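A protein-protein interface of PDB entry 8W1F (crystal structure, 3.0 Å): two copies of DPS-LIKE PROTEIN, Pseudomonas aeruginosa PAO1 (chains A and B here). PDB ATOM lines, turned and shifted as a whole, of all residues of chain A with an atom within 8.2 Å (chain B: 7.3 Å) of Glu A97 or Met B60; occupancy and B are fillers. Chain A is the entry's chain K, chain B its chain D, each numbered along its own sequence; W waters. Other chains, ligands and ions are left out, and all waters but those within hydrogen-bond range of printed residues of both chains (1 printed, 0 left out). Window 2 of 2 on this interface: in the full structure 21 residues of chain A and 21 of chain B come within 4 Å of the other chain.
The side-chain carboxylate (OE1) of Glu A97 lies within salt-bridge range of the guanidinium group (NH2) of Arg B56 (2.9 Å). The backbone carbonyl oxygen of Pro A98 sits at hydrogen-bond distance from the guanidinium group of Arg B56, at 2.9 Å. The backbone carbonyl oxygen (O) of Phe B59 lies close to the side-chain sulfur (SD) of Met A92, at 3.6 Å. The side-chain sulfur (SD) of Met B60 lies close to the side-chain sulfur (SD) of Met A92 (3.8 Å).
Water W1 lies within hydrogen-bond range of OE2 of Glu B115 (3.2 Å) and OE1 of Glu A97 (3.4 Å).
Of chain A, only Met A92 (3.8 Å) and Glu A97 (3.5 Å) come within 4 Å of Met B60. Printed residues of chain B within 4 Å of Met A92: Phe B59 and Met B60. Printed residues of chain B within 4 Å of Pro A98: Arg B56 and Phe B59. Of the printed residues of chain A, Arg B56 touches Glu A97, Pro A98 and Phe A100. Printed residues of chain B within 4 Å of Ala A88: Phe B59. Of the printed residues of chain A, Phe B59 touches Ala A88 (3.6 Å), Met A92 (2.8 Å), Pro A98 (3.98 Å) and Phe A100 (3.7 Å). Tyr B54 touches none of the printed residues of chain A. The nearest residue of chain B that does not touch Glu A97 is Glu B115 (4.5 Å). The nearest residue of chain A that does not touch Met B60 is Pro A98 (4.1 Å). The nearest printed residue of chain B that does not touch Ala A88 is Lys B55 (6.8 Å).
Of the 18 printed residues of chain A, 5 touch a printed residue of chain B. Hydrophobic or aromatic side chains of chain B within 4 Å of the printed part of chain A: Phe B59 and Met B60. Among the printed residues, Asp or Glu carboxylates within 4 Å of a Lys or Arg side-chain nitrogen of the other chain: Glu A97 with Arg B56.
No position is printed for both chains.
Among the printed residues, merely in contact across the chains: Glu A97 with Met B60, Ala A88 with Phe B59, Phe A100 with Phe B59, Phe A100 with Arg B56 and Pro A98 with Phe B59.
The guanidinium group (NH2) of Arg B56 lies within salt-bridge range of the side-chain carboxylate (OE1) of Glu B115, 3.4 Å away. O of Glu A97 is in hydrogen-bond range of ND2 of Asn A41.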
ATOM      1  N   ARG A  33       3.616  -0.369   7.287  1.00  0.00           N
ATOM      2  CA  ARG A  33       2.369   0.391   7.290  1.00  0.00           C
ATOM      3  C   ARG A  33       1.277  -0.327   8.080  1.00  0.00           C
ATOM      4  O   ARG A  33       0.536   0.297   8.847  1.00  0.00           O
ATOM      5  CB  ARG A  33       1.923   0.631   5.842  1.00  0.00           C
ATOM      6  CG  ARG A  33       0.831   1.669   5.642  1.00  0.00           C
ATOM      7  CD  ARG A  33       0.419   1.766   4.176  1.00  0.00           C
ATOM      8  NE  ARG A  33      -0.130   0.484   3.754  1.00  0.00           N
ATOM      9  CZ  ARG A  33      -1.389   0.110   3.946  1.00  0.00           C
ATOM     10  NH1 ARG A  33      -2.278   0.924   4.488  1.00  0.00           N
ATOM     11  NH2 ARG A  33      -1.759  -1.125   3.616  1.00  0.00           N
ATOM     12  N   LEU A  37      -0.374   1.322  11.491  1.00  0.00           N
ATOM     13  CA  LEU A  37      -1.813   1.521  11.589  1.00  0.00           C
ATOM     14  C   LEU A  37      -2.372   0.855  12.843  1.00  0.00           C
ATOM     15  O   LEU A  37      -3.256   1.406  13.506  1.00  0.00           O
ATOM     16  CB  LEU A  37      -2.508   0.982  10.340  1.00  0.00           C
ATOM     17  CG  LEU A  37      -2.385   1.866   9.096  1.00  0.00           C
ATOM     18  CD1 LEU A  37      -3.029   1.179   7.924  1.00  0.00           C
ATOM     19  CD2 LEU A  37      -2.968   3.258   9.308  1.00  0.00           C
ATOM     20  N   LEU A  40      -1.425   3.138  15.745  1.00  0.00           N
ATOM     21  CA  LEU A  40      -2.197   4.376  15.751  1.00  0.00           C
ATOM     22  C   LEU A  40      -3.595   4.134  16.302  1.00  0.00           C
ATOM     23  O   LEU A  40      -4.126   4.961  17.052  1.00  0.00           O
ATOM     24  CB  LEU A  40      -2.281   4.964  14.343  1.00  0.00           C
ATOM     25  CG  LEU A  40      -0.983   5.553  13.787  1.00  0.00           C
ATOM     26  CD1 LEU A  40      -1.121   5.853  12.313  1.00  0.00           C
ATOM     27  CD2 LEU A  40      -0.593   6.785  14.548  1.00  0.00           C
ATOM     28  N   ASN A  41      -4.216   3.012  15.929  1.00  0.00           N
ATOM     29  CA  ASN A  41      -5.563   2.730  16.408  1.00  0.00           C
ATOM     30  C   ASN A  41      -5.573   2.399  17.894  1.00  0.00           C
ATOM     31  O   ASN A  41      -6.533   2.748  18.594  1.00  0.00           O
ATOM     32  CB  ASN A  41      -6.184   1.588  15.606  1.00  0.00           C
ATOM     33  CG  ASN A  41      -7.160   2.080  14.523  1.00  0.00           C
ATOM     34  OD1 ASN A  41      -8.067   2.865  14.775  1.00  0.00           O
ATOM     35  ND2 ASN A  41      -6.967   1.598  13.309  1.00  0.00           N
ATOM     36  N   LEU A  44      -5.376   5.693  19.501  1.00  0.00           N
ATOM     37  CA  LEU A  44      -6.660   6.369  19.373  1.00  0.00           C
ATOM     38  C   LEU A  44      -7.640   5.862  20.424  1.00  0.00           C
ATOM     39  O   LEU A  44      -8.393   6.648  21.015  1.00  0.00           O
ATOM     40  CB  LEU A  44      -7.215   6.170  17.964  1.00  0.00           C
ATOM     41  CG  LEU A  44      -8.635   6.687  17.718  1.00  0.00           C
ATOM     42  CD1 LEU A  44      -8.746   8.160  18.049  1.00  0.00           C
ATOM     43  CD2 LEU A  44      -9.056   6.440  16.281  1.00  0.00           C
ATOM     44  N   LEU A  87      -4.253  11.521  15.694  1.00  0.00           N
ATOM     45  CA  LEU A  87      -3.982  10.128  15.354  1.00  0.00           C
ATOM     46  C   LEU A  87      -4.924   9.625  14.263  1.00  0.00           C
ATOM     47  O   LEU A  87      -4.483   8.964  13.314  1.00  0.00           O
ATOM     48  CB  LEU A  87      -4.092   9.250  16.607  1.00  0.00           C
ATOM     49  CG  LEU A  87      -3.128   9.533  17.766  1.00  0.00           C
ATOM     50  CD1 LEU A  87      -3.663   8.919  19.042  1.00  0.00           C
ATOM     51  CD2 LEU A  87      -1.743   8.990  17.493  1.00  0.00           C
ATOM     52  N   ALA A  88      -6.220   9.928  14.377  1.00  0.00           N
ATOM     53  CA  ALA A  88      -7.180   9.454  13.386  1.00  0.00           C
ATOM     54  C   ALA A  88      -6.862  10.001  11.998  1.00  0.00           C
ATOM     55  O   ALA A  88      -6.949   9.279  10.993  1.00  0.00           O
ATOM     56  CB  ALA A  88      -8.592   9.846  13.805  1.00  0.00           C
ATOM     57  N   ARG A  90      -3.978  10.698  10.831  1.00  0.00           N
ATOM     58  CA  ARG A  90      -2.830   9.960  10.316  1.00  0.00           C
ATOM     59  C   ARG A  90      -3.229   8.549   9.897  1.00  0.00           C
ATOM     60  O   ARG A  90      -2.637   7.977   8.973  1.00  0.00           O
ATOM     61  CB  ARG A  90      -1.725   9.910  11.367  1.00  0.00           C
ATOM     62  CG  ARG A  90      -0.409   9.319  10.867  1.00  0.00           C
ATOM     63  CD  ARG A  90       0.124  10.110   9.685  1.00  0.00           C
ATOM     64  NE  ARG A  90       1.423   9.640   9.224  1.00  0.00           N
ATOM     65  CZ  ARG A  90       1.946   9.952   8.048  1.00  0.00           C
ATOM     66  NH1 ARG A  90       1.297  10.719   7.194  1.00  0.00           N
ATOM     67  NH2 ARG A  90       3.145   9.477   7.722  1.00  0.00           N
ATOM     68  N   ILE A  91      -4.201   7.959  10.592  1.00  0.00           N
ATOM     69  CA  ILE A  91      -4.707   6.652  10.192  1.00  0.00           C
ATOM     70  C   ILE A  91      -5.267   6.732   8.782  1.00  0.00           C
ATOM     71  O   ILE A  91      -4.991   5.878   7.937  1.00  0.00           O
ATOM     72  CB  ILE A  91      -5.752   6.156  11.212  1.00  0.00           C
ATOM     73  CG1 ILE A  91      -5.045   5.760  12.524  1.00  0.00           C
ATOM     74  CG2 ILE A  91      -6.560   5.001  10.640  1.00  0.00           C
ATOM     75  CD1 ILE A  91      -5.975   5.516  13.715  1.00  0.00           C
ATOM     76  N   MET A  92      -6.031   7.784   8.493  1.00  0.00           N
ATOM     77  CA  MET A  92      -6.563   7.950   7.148  1.00  0.00           C
ATOM     78  C   MET A  92      -5.441   8.120   6.131  1.00  0.00           C
ATOM     79  O   MET A  92      -5.463   7.493   5.065  1.00  0.00           O
ATOM     80  CB  MET A  92      -7.505   9.149   7.104  1.00  0.00           C
ATOM     81  CG  MET A  92      -8.741   9.007   7.970  1.00  0.00           C
ATOM     82  SD  MET A  92      -9.753   7.610   7.472  1.00  0.00           S
ATOM     83  CE  MET A  92     -10.304   8.161   5.906  1.00  0.00           C
ATOM     84  N   GLN A  93      -4.434   8.939   6.453  1.00  0.00           N
ATOM     85  CA  GLN A  93      -3.373   9.211   5.490  1.00  0.00           C
ATOM     86  C   GLN A  93      -2.603   7.950   5.120  1.00  0.00           C
ATOM     87  O   GLN A  93      -2.151   7.802   3.978  1.00  0.00           O
ATOM     88  CB  GLN A  93      -2.398  10.246   6.039  1.00  0.00           C
ATOM     89  CG  GLN A  93      -3.017  11.578   6.214  1.00  0.00           C
ATOM     90  CD  GLN A  93      -2.103  12.545   6.881  1.00  0.00           C
ATOM     91  OE1 GLN A  93      -1.005  12.197   7.296  1.00  0.00           O
ATOM     92  NE2 GLN A  93      -2.561  13.772   7.012  1.00  0.00           N
ATOM     93  N   LEU A  94      -2.401   7.057   6.085  1.00  0.00           N
ATOM     94  CA  LEU A  94      -1.675   5.815   5.870  1.00  0.00           C
ATOM     95  C   LEU A  94      -2.593   4.711   5.390  1.00  0.00           C
ATOM     96  O   LEU A  94      -2.197   3.545   5.394  1.00  0.00           O
ATOM     97  CB  LEU A  94      -0.970   5.392   7.157  1.00  0.00           C
ATOM     98  CG  LEU A  94       0.145   6.322   7.645  1.00  0.00           C
ATOM     99  CD1 LEU A  94       0.698   5.881   8.989  1.00  0.00           C
ATOM    100  CD2 LEU A  94       1.276   6.366   6.655  1.00  0.00           C
ATOM    101  N   GLY A  95      -3.828   5.047   5.036  1.00  0.00           N
ATOM    102  CA  GLY A  95      -4.702   4.105   4.377  1.00  0.00           C
ATOM    103  C   GLY A  95      -5.487   3.181   5.271  1.00  0.00           C
ATOM    104  O   GLY A  95      -5.921   2.123   4.801  1.00  0.00           O
ATOM    105  N   GLY A  96      -5.681   3.535   6.542  1.00  0.00           N
ATOM    106  CA  GLY A  96      -6.461   2.736   7.459  1.00  0.00           C
ATOM    107  C   GLY A  96      -7.836   3.331   7.715  1.00  0.00           C
ATOM    108  O   GLY A  96      -8.322   4.202   6.990  1.00  0.00           O
ATOM    109  N   GLU A  97      -8.485   2.814   8.754  1.00  0.00           N
ATOM    110  CA  GLU A  97      -9.792   3.298   9.187  1.00  0.00           C
ATOM    111  C   GLU A  97      -9.723   3.509  10.691  1.00  0.00           C
ATOM    112  O   GLU A  97      -9.485   2.539  11.438  1.00  0.00           O
ATOM    113  CB  GLU A  97     -10.892   2.295   8.838  1.00  0.00           C
ATOM    114  CG  GLU A  97     -11.002   1.959   7.372  1.00  0.00           C
ATOM    115  CD  GLU A  97     -12.091   0.941   7.099  1.00  0.00           C
ATOM    116  OE1 GLU A  97     -12.711   0.488   8.092  1.00  0.00           O
ATOM    117  OE2 GLU A  97     -12.308   0.591   5.908  1.00  0.00           O
ATOM    118  N   PRO A  98     -10.001   4.704  11.193  1.00  0.00           N
ATOM    119  CA  PRO A  98      -9.920   4.923  12.643  1.00  0.00           C
ATOM    120  C   PRO A  98     -11.141   4.342  13.341  1.00  0.00           C
ATOM    121  O   PRO A  98     -12.278   4.643  12.976  1.00  0.00           O
ATOM    122  CB  PRO A  98      -9.869   6.451  12.766  1.00  0.00           C
ATOM    123  CG  PRO A  98     -10.656   6.924  11.583  1.00  0.00           C
ATOM    124  CD  PRO A  98     -10.395   5.925  10.469  1.00  0.00           C
ATOM    125  N   ASP A  99     -10.903   3.528  14.366  1.00  0.00           N
ATOM    126  CA  ASP A  99     -11.966   2.779  15.028  1.00  0.00           C
ATOM    127  C   ASP A  99     -12.455   3.541  16.252  1.00  0.00           C
ATOM    128  O   ASP A  99     -11.820   3.516  17.304  1.00  0.00           O
ATOM    129  CB  ASP A  99     -11.467   1.389  15.410  1.00  0.00           C
ATOM    130  CG  ASP A  99     -12.577   0.497  15.907  1.00  0.00           C
ATOM    131  OD1 ASP A  99     -13.732   0.978  15.927  1.00  0.00           O
ATOM    132  OD2 ASP A  99     -12.307  -0.685  16.235  1.00  0.00           O
ATOM    133  N   PHE A 100     -13.617   4.180  16.123  1.00  0.00           N
ATOM    134  CA  PHE A 100     -14.267   4.880  17.219  1.00  0.00           C
ATOM    135  C   PHE A 100     -15.349   4.036  17.897  1.00  0.00           C
ATOM    136  O   PHE A 100     -16.136   4.568  18.688  1.00  0.00           O
ATOM    137  CB  PHE A 100     -14.897   6.190  16.716  1.00  0.00           C
ATOM    138  CG  PHE A 100     -13.902   7.256  16.325  1.00  0.00           C
ATOM    139  CD1 PHE A 100     -13.318   7.255  15.067  1.00  0.00           C
ATOM    140  CD2 PHE A 100     -13.567   8.269  17.212  1.00  0.00           C
ATOM    141  CE1 PHE A 100     -12.409   8.239  14.717  1.00  0.00           C
ATOM    142  CE2 PHE A 100     -12.661   9.254  16.865  1.00  0.00           C
ATOM    143  CZ  PHE A 100     -12.085   9.242  15.622  1.00  0.00           C
ATOM    144  N   TYR B  54     -20.518  10.109  14.403  1.00  0.00           N
ATOM    145  CA  TYR B  54     -20.274  11.206  13.480  1.00  0.00           C
ATOM    146  C   TYR B  54     -18.780  11.406  13.245  1.00  0.00           C
ATOM    147  O   TYR B  54     -18.364  11.706  12.124  1.00  0.00           O
ATOM    148  CB  TYR B  54     -20.912  12.487  14.002  1.00  0.00           C
ATOM    149  CG  TYR B  54     -22.345  12.739  13.557  1.00  0.00           C
ATOM    150  CD1 TYR B  54     -22.677  12.836  12.210  1.00  0.00           C
ATOM    151  CD2 TYR B  54     -23.346  12.970  14.491  1.00  0.00           C
ATOM    152  CE1 TYR B  54     -23.974  13.108  11.812  1.00  0.00           C
ATOM    153  CE2 TYR B  54     -24.631  13.253  14.102  1.00  0.00           C
ATOM    154  CZ  TYR B  54     -24.943  13.325  12.763  1.00  0.00           C
ATOM    155  OH  TYR B  54     -26.233  13.604  12.369  1.00  0.00           O
ATOM    156  N   LYS B  55     -17.956  11.265  14.287  1.00  0.00           N
ATOM    157  CA  LYS B  55     -16.516  11.417  14.084  1.00  0.00           C
ATOM    158  C   LYS B  55     -15.977  10.344  13.140  1.00  0.00           C
ATOM    159  O   LYS B  55     -15.136  10.627  12.280  1.00  0.00           O
ATOM    160  CB  LYS B  55     -15.777  11.386  15.422  1.00  0.00           C
ATOM    161  CG  LYS B  55     -15.835  12.703  16.201  1.00  0.00           C
ATOM    162  CD  LYS B  55     -15.083  13.836  15.497  1.00  0.00           C
ATOM    163  CE  LYS B  55     -13.657  13.942  15.998  1.00  0.00           C
ATOM    164  NZ  LYS B  55     -13.625  14.765  17.216  1.00  0.00           N
ATOM    165  N   ARG B  56     -16.434   9.102  13.301  1.00  0.00           N
ATOM    166  CA  ARG B  56     -16.065   8.046  12.363  1.00  0.00           C
ATOM    167  C   ARG B  56     -16.433   8.446  10.941  1.00  0.00           C
ATOM    168  O   ARG B  56     -15.605   8.362  10.025  1.00  0.00           O
ATOM    169  CB  ARG B  56     -16.753   6.737  12.756  1.00  0.00           C
ATOM    170  CG  ARG B  56     -16.758   5.675  11.681  1.00  0.00           C
ATOM    171  CD  ARG B  56     -15.408   5.026  11.480  1.00  0.00           C
ATOM    172  NE  ARG B  56     -15.488   4.009  10.441  1.00  0.00           N
ATOM    173  CZ  ARG B  56     -14.602   3.039  10.259  1.00  0.00           C
ATOM    174  NH1 ARG B  56     -13.555   2.897  11.054  1.00  0.00           N
ATOM    175  NH2 ARG B  56     -14.780   2.178   9.261  1.00  0.00           N
ATOM    176  N   HIS B  57     -17.679   8.890  10.742  1.00  0.00           N
ATOM    177  CA  HIS B  57     -18.130   9.290   9.414  1.00  0.00           C
ATOM    178  C   HIS B  57     -17.343  10.480   8.875  1.00  0.00           C
ATOM    179  O   HIS B  57     -16.996  10.524   7.687  1.00  0.00           O
ATOM    180  CB  HIS B  57     -19.618   9.615   9.465  1.00  0.00           C
ATOM    181  CG  HIS B  57     -20.468   8.428   9.768  1.00  0.00           C
ATOM    182  ND1 HIS B  57     -21.808   8.526  10.066  1.00  0.00           N
ATOM    183  CD2 HIS B  57     -20.174   7.107   9.769  1.00  0.00           C
ATOM    184  CE1 HIS B  57     -22.299   7.316  10.265  1.00  0.00           C
ATOM    185  NE2 HIS B  57     -21.328   6.438  10.091  1.00  0.00           N
ATOM    186  N   TYR B  58     -17.025  11.437   9.739  1.00  0.00           N
ATOM    187  CA  TYR B  58     -16.269  12.597   9.299  1.00  0.00           C
ATOM    188  C   TYR B  58     -14.961  12.191   8.641  1.00  0.00           C
ATOM    189  O   TYR B  58     -14.623  12.674   7.551  1.00  0.00           O
ATOM    190  CB  TYR B  58     -16.001  13.498  10.490  1.00  0.00           C
ATOM    191  CG  TYR B  58     -14.873  14.461  10.254  1.00  0.00           C
ATOM    192  CD1 TYR B  58     -15.004  15.515   9.374  1.00  0.00           C
ATOM    193  CD2 TYR B  58     -13.667  14.296  10.896  1.00  0.00           C
ATOM    194  CE1 TYR B  58     -13.979  16.382   9.162  1.00  0.00           C
ATOM    195  CE2 TYR B  58     -12.642  15.159  10.684  1.00  0.00           C
ATOM    196  CZ  TYR B  58     -12.806  16.198   9.821  1.00  0.00           C
ATOM    197  OH  TYR B  58     -11.775  17.062   9.613  1.00  0.00           O
ATOM    198  N   PHE B  59     -14.200  11.309   9.293  1.00  0.00           N
ATOM    199  CA  PHE B  59     -12.888  10.950   8.767  1.00  0.00           C
ATOM    200  C   PHE B  59     -12.994  10.091   7.514  1.00  0.00           C
ATOM    201  O   PHE B  59     -12.121  10.166   6.636  1.00  0.00           O
ATOM    202  CB  PHE B  59     -12.076  10.214   9.840  1.00  0.00           C
ATOM    203  CG  PHE B  59     -11.563  11.109  10.951  1.00  0.00           C
ATOM    204  CD1 PHE B  59     -10.443  11.905  10.764  1.00  0.00           C
ATOM    205  CD2 PHE B  59     -12.199  11.146  12.177  1.00  0.00           C
ATOM    206  CE1 PHE B  59      -9.975  12.711  11.770  1.00  0.00           C
ATOM    207  CE2 PHE B  59     -11.728  11.958  13.187  1.00  0.00           C
ATOM    208  CZ  PHE B  59     -10.613  12.739  12.982  1.00  0.00           C
ATOM    209  N   MET B  60     -14.049   9.284   7.409  1.00  0.00           N
ATOM    210  CA  MET B  60     -14.174   8.317   6.332  1.00  0.00           C
ATOM    211  C   MET B  60     -14.865   8.860   5.097  1.00  0.00           C
ATOM    212  O   MET B  60     -14.779   8.229   4.043  1.00  0.00           O
ATOM    213  CB  MET B  60     -14.942   7.099   6.828  1.00  0.00           C
ATOM    214  CG  MET B  60     -14.177   6.289   7.848  1.00  0.00           C
ATOM    215  SD  MET B  60     -12.794   5.411   7.123  1.00  0.00           S
ATOM    216  CE  MET B  60     -13.674   4.053   6.370  1.00  0.00           C
ATOM    217  N   ALA B  61     -15.538  10.004   5.191  1.00  0.00           N
ATOM    218  CA  ALA B  61     -16.320  10.525   4.073  1.00  0.00           C
ATOM    219  C   ALA B  61     -15.424  11.377   3.189  1.00  0.00           C
ATOM    220  O   ALA B  61     -15.449  12.609   3.231  1.00  0.00           O
ATOM    221  CB  ALA B  61     -17.502  11.338   4.574  1.00  0.00           C
ATOM    222  N   THR B  62     -14.647  10.702   2.348  1.00  0.00           N
ATOM    223  CA  THR B  62     -13.705  11.379   1.472  1.00  0.00           C
ATOM    224  C   THR B  62     -14.229  11.447   0.038  1.00  0.00           C
ATOM    225  O   THR B  62     -14.965  10.569  -0.425  1.00  0.00           O
ATOM    226  CB  THR B  62     -12.339  10.687   1.475  1.00  0.00           C
ATOM    227  OG1 THR B  62     -12.412   9.486   0.700  1.00  0.00           O
ATOM    228  CG2 THR B  62     -11.898  10.348   2.870  1.00  0.00           C
ATOM    229  N   GLY B  63     -13.788  12.474  -0.659  1.00  0.00           N
ATOM    230  CA  GLY B  63     -14.206  12.811  -2.024  1.00  0.00           C
ATOM    231  C   GLY B  63     -14.859  14.183  -2.000  1.00  0.00           C
ATOM    232  O   GLY B  63     -15.259  14.719  -1.000  1.00  0.00           O
ATOM    233  N   ALA B  66     -18.562  14.029  -0.988  1.00  0.00           N
ATOM    234  CA  ALA B  66     -18.576  13.515   0.373  1.00  0.00           C
ATOM    235  C   ALA B  66     -17.999  14.517   1.358  1.00  0.00           C
ATOM    236  O   ALA B  66     -18.413  14.540   2.522  1.00  0.00           O
ATOM    237  CB  ALA B  66     -17.784  12.214   0.454  1.00  0.00           C
ATOM    238  N   ALA B  70     -19.013  15.447   5.084  1.00  0.00           N
ATOM    239  CA  ALA B  70     -18.078  15.324   6.198  1.00  0.00           C
ATOM    240  C   ALA B  70     -18.120  16.559   7.087  1.00  0.00           C
ATOM    241  O   ALA B  70     -18.075  16.454   8.318  1.00  0.00           O
ATOM    242  CB  ALA B  70     -16.661  15.094   5.669  1.00  0.00           C
ATOM    243  N   PHE B  73     -21.059  16.294   9.201  1.00  0.00           N
ATOM    244  CA  PHE B  73     -20.845  15.252  10.201  1.00  0.00           C
ATOM    245  C   PHE B  73     -20.046  15.804  11.371  1.00  0.00           C
ATOM    246  O   PHE B  73     -20.368  15.553  12.536  1.00  0.00           O
ATOM    247  CB  PHE B  73     -20.111  14.049   9.601  1.00  0.00           C
ATOM    248  CG  PHE B  73     -20.897  13.287   8.566  1.00  0.00           C
ATOM    249  CD1 PHE B  73     -22.277  13.365   8.501  1.00  0.00           C
ATOM    250  CD2 PHE B  73     -20.238  12.522   7.624  1.00  0.00           C
ATOM    251  CE1 PHE B  73     -22.981  12.673   7.526  1.00  0.00           C
ATOM    252  CE2 PHE B  73     -20.937  11.839   6.661  1.00  0.00           C
ATOM    253  CZ  PHE B  73     -22.311  11.914   6.612  1.00  0.00           C
ATOM    254  N   GLU B 115     -20.655   1.894  11.446  1.00  0.00           N
ATOM    255  CA  GLU B 115     -19.582   2.437  10.620  1.00  0.00           C
ATOM    256  C   GLU B 115     -20.105   2.861   9.255  1.00  0.00           C
ATOM    257  O   GLU B 115     -19.714   3.917   8.732  1.00  0.00           O
ATOM    258  CB  GLU B 115     -18.453   1.409  10.438  1.00  0.00           C
ATOM    259  CG  GLU B 115     -17.635   1.082  11.688  1.00  0.00           C
ATOM    260  CD  GLU B 115     -16.468   0.125  11.412  1.00  0.00           C
ATOM    261  OE1 GLU B 115     -16.483  -0.539  10.341  1.00  0.00           O
ATOM    262  OE2 GLU B 115     -15.542   0.053  12.269  1.00  0.00           O
ATOM    263  N   GLY B 116     -20.957   2.028   8.649  1.00  0.00           N
ATOM    264  CA  GLY B 116     -21.396   2.217   7.277  1.00  0.00           C
ATOM    265  C   GLY B 116     -20.328   1.889   6.250  1.00  0.00           C
ATOM    266  O   GLY B 116     -19.134   2.085   6.500  1.00  0.00           O
ATOM    267  N   LYS B 117     -20.735   1.412   5.080  1.00  0.00           N
ATOM    268  CA  LYS B 117     -19.787   1.113   4.012  1.00  0.00           C
ATOM    269  C   LYS B 117     -19.759   2.212   2.958  1.00  0.00           C
ATOM    270  O   LYS B 117     -18.688   2.539   2.452  1.00  0.00           O
ATOM    271  CB  LYS B 117     -20.103  -0.243   3.374  1.00  0.00           C
ATOM    272  N   LEU B 119     -21.322   6.254   1.514  1.00  0.00           N
ATOM    273  CA  LEU B 119     -21.798   7.528   2.033  1.00  0.00           C
ATOM    274  C   LEU B 119     -23.278   7.445   2.344  1.00  0.00           C
ATOM    275  O   LEU B 119     -23.725   7.906   3.400  1.00  0.00           O
ATOM    276  CB  LEU B 119     -21.544   8.648   1.027  1.00  0.00           C
ATOM    277  CG  LEU B 119     -22.041  10.045   1.409  1.00  0.00           C
ATOM    278  CD1 LEU B 119     -21.306  10.550   2.653  1.00  0.00           C
ATOM    279  CD2 LEU B 119     -21.903  11.034   0.254  1.00  0.00           C
ATOM    280  N   MET B 122     -23.759   5.942   5.669  1.00  0.00           N
ATOM    281  CA  MET B 122     -23.455   6.853   6.767  1.00  0.00           C
ATOM    282  C   MET B 122     -24.594   7.843   6.978  1.00  0.00           C
ATOM    283  O   MET B 122     -25.081   8.015   8.100  1.00  0.00           O
ATOM    284  CB  MET B 122     -22.127   7.571   6.487  1.00  0.00           C
ATOM    285  CG  MET B 122     -20.957   6.600   6.347  1.00  0.00           C
ATOM    286  SD  MET B 122     -19.300   7.277   6.051  1.00  0.00           S
ATOM    287  CE  MET B 122     -19.674   8.740   5.153  1.00  0.00           C
HETATM  288  O   HOH W   1     -12.685  -0.800  11.193  1.00  0.00           O
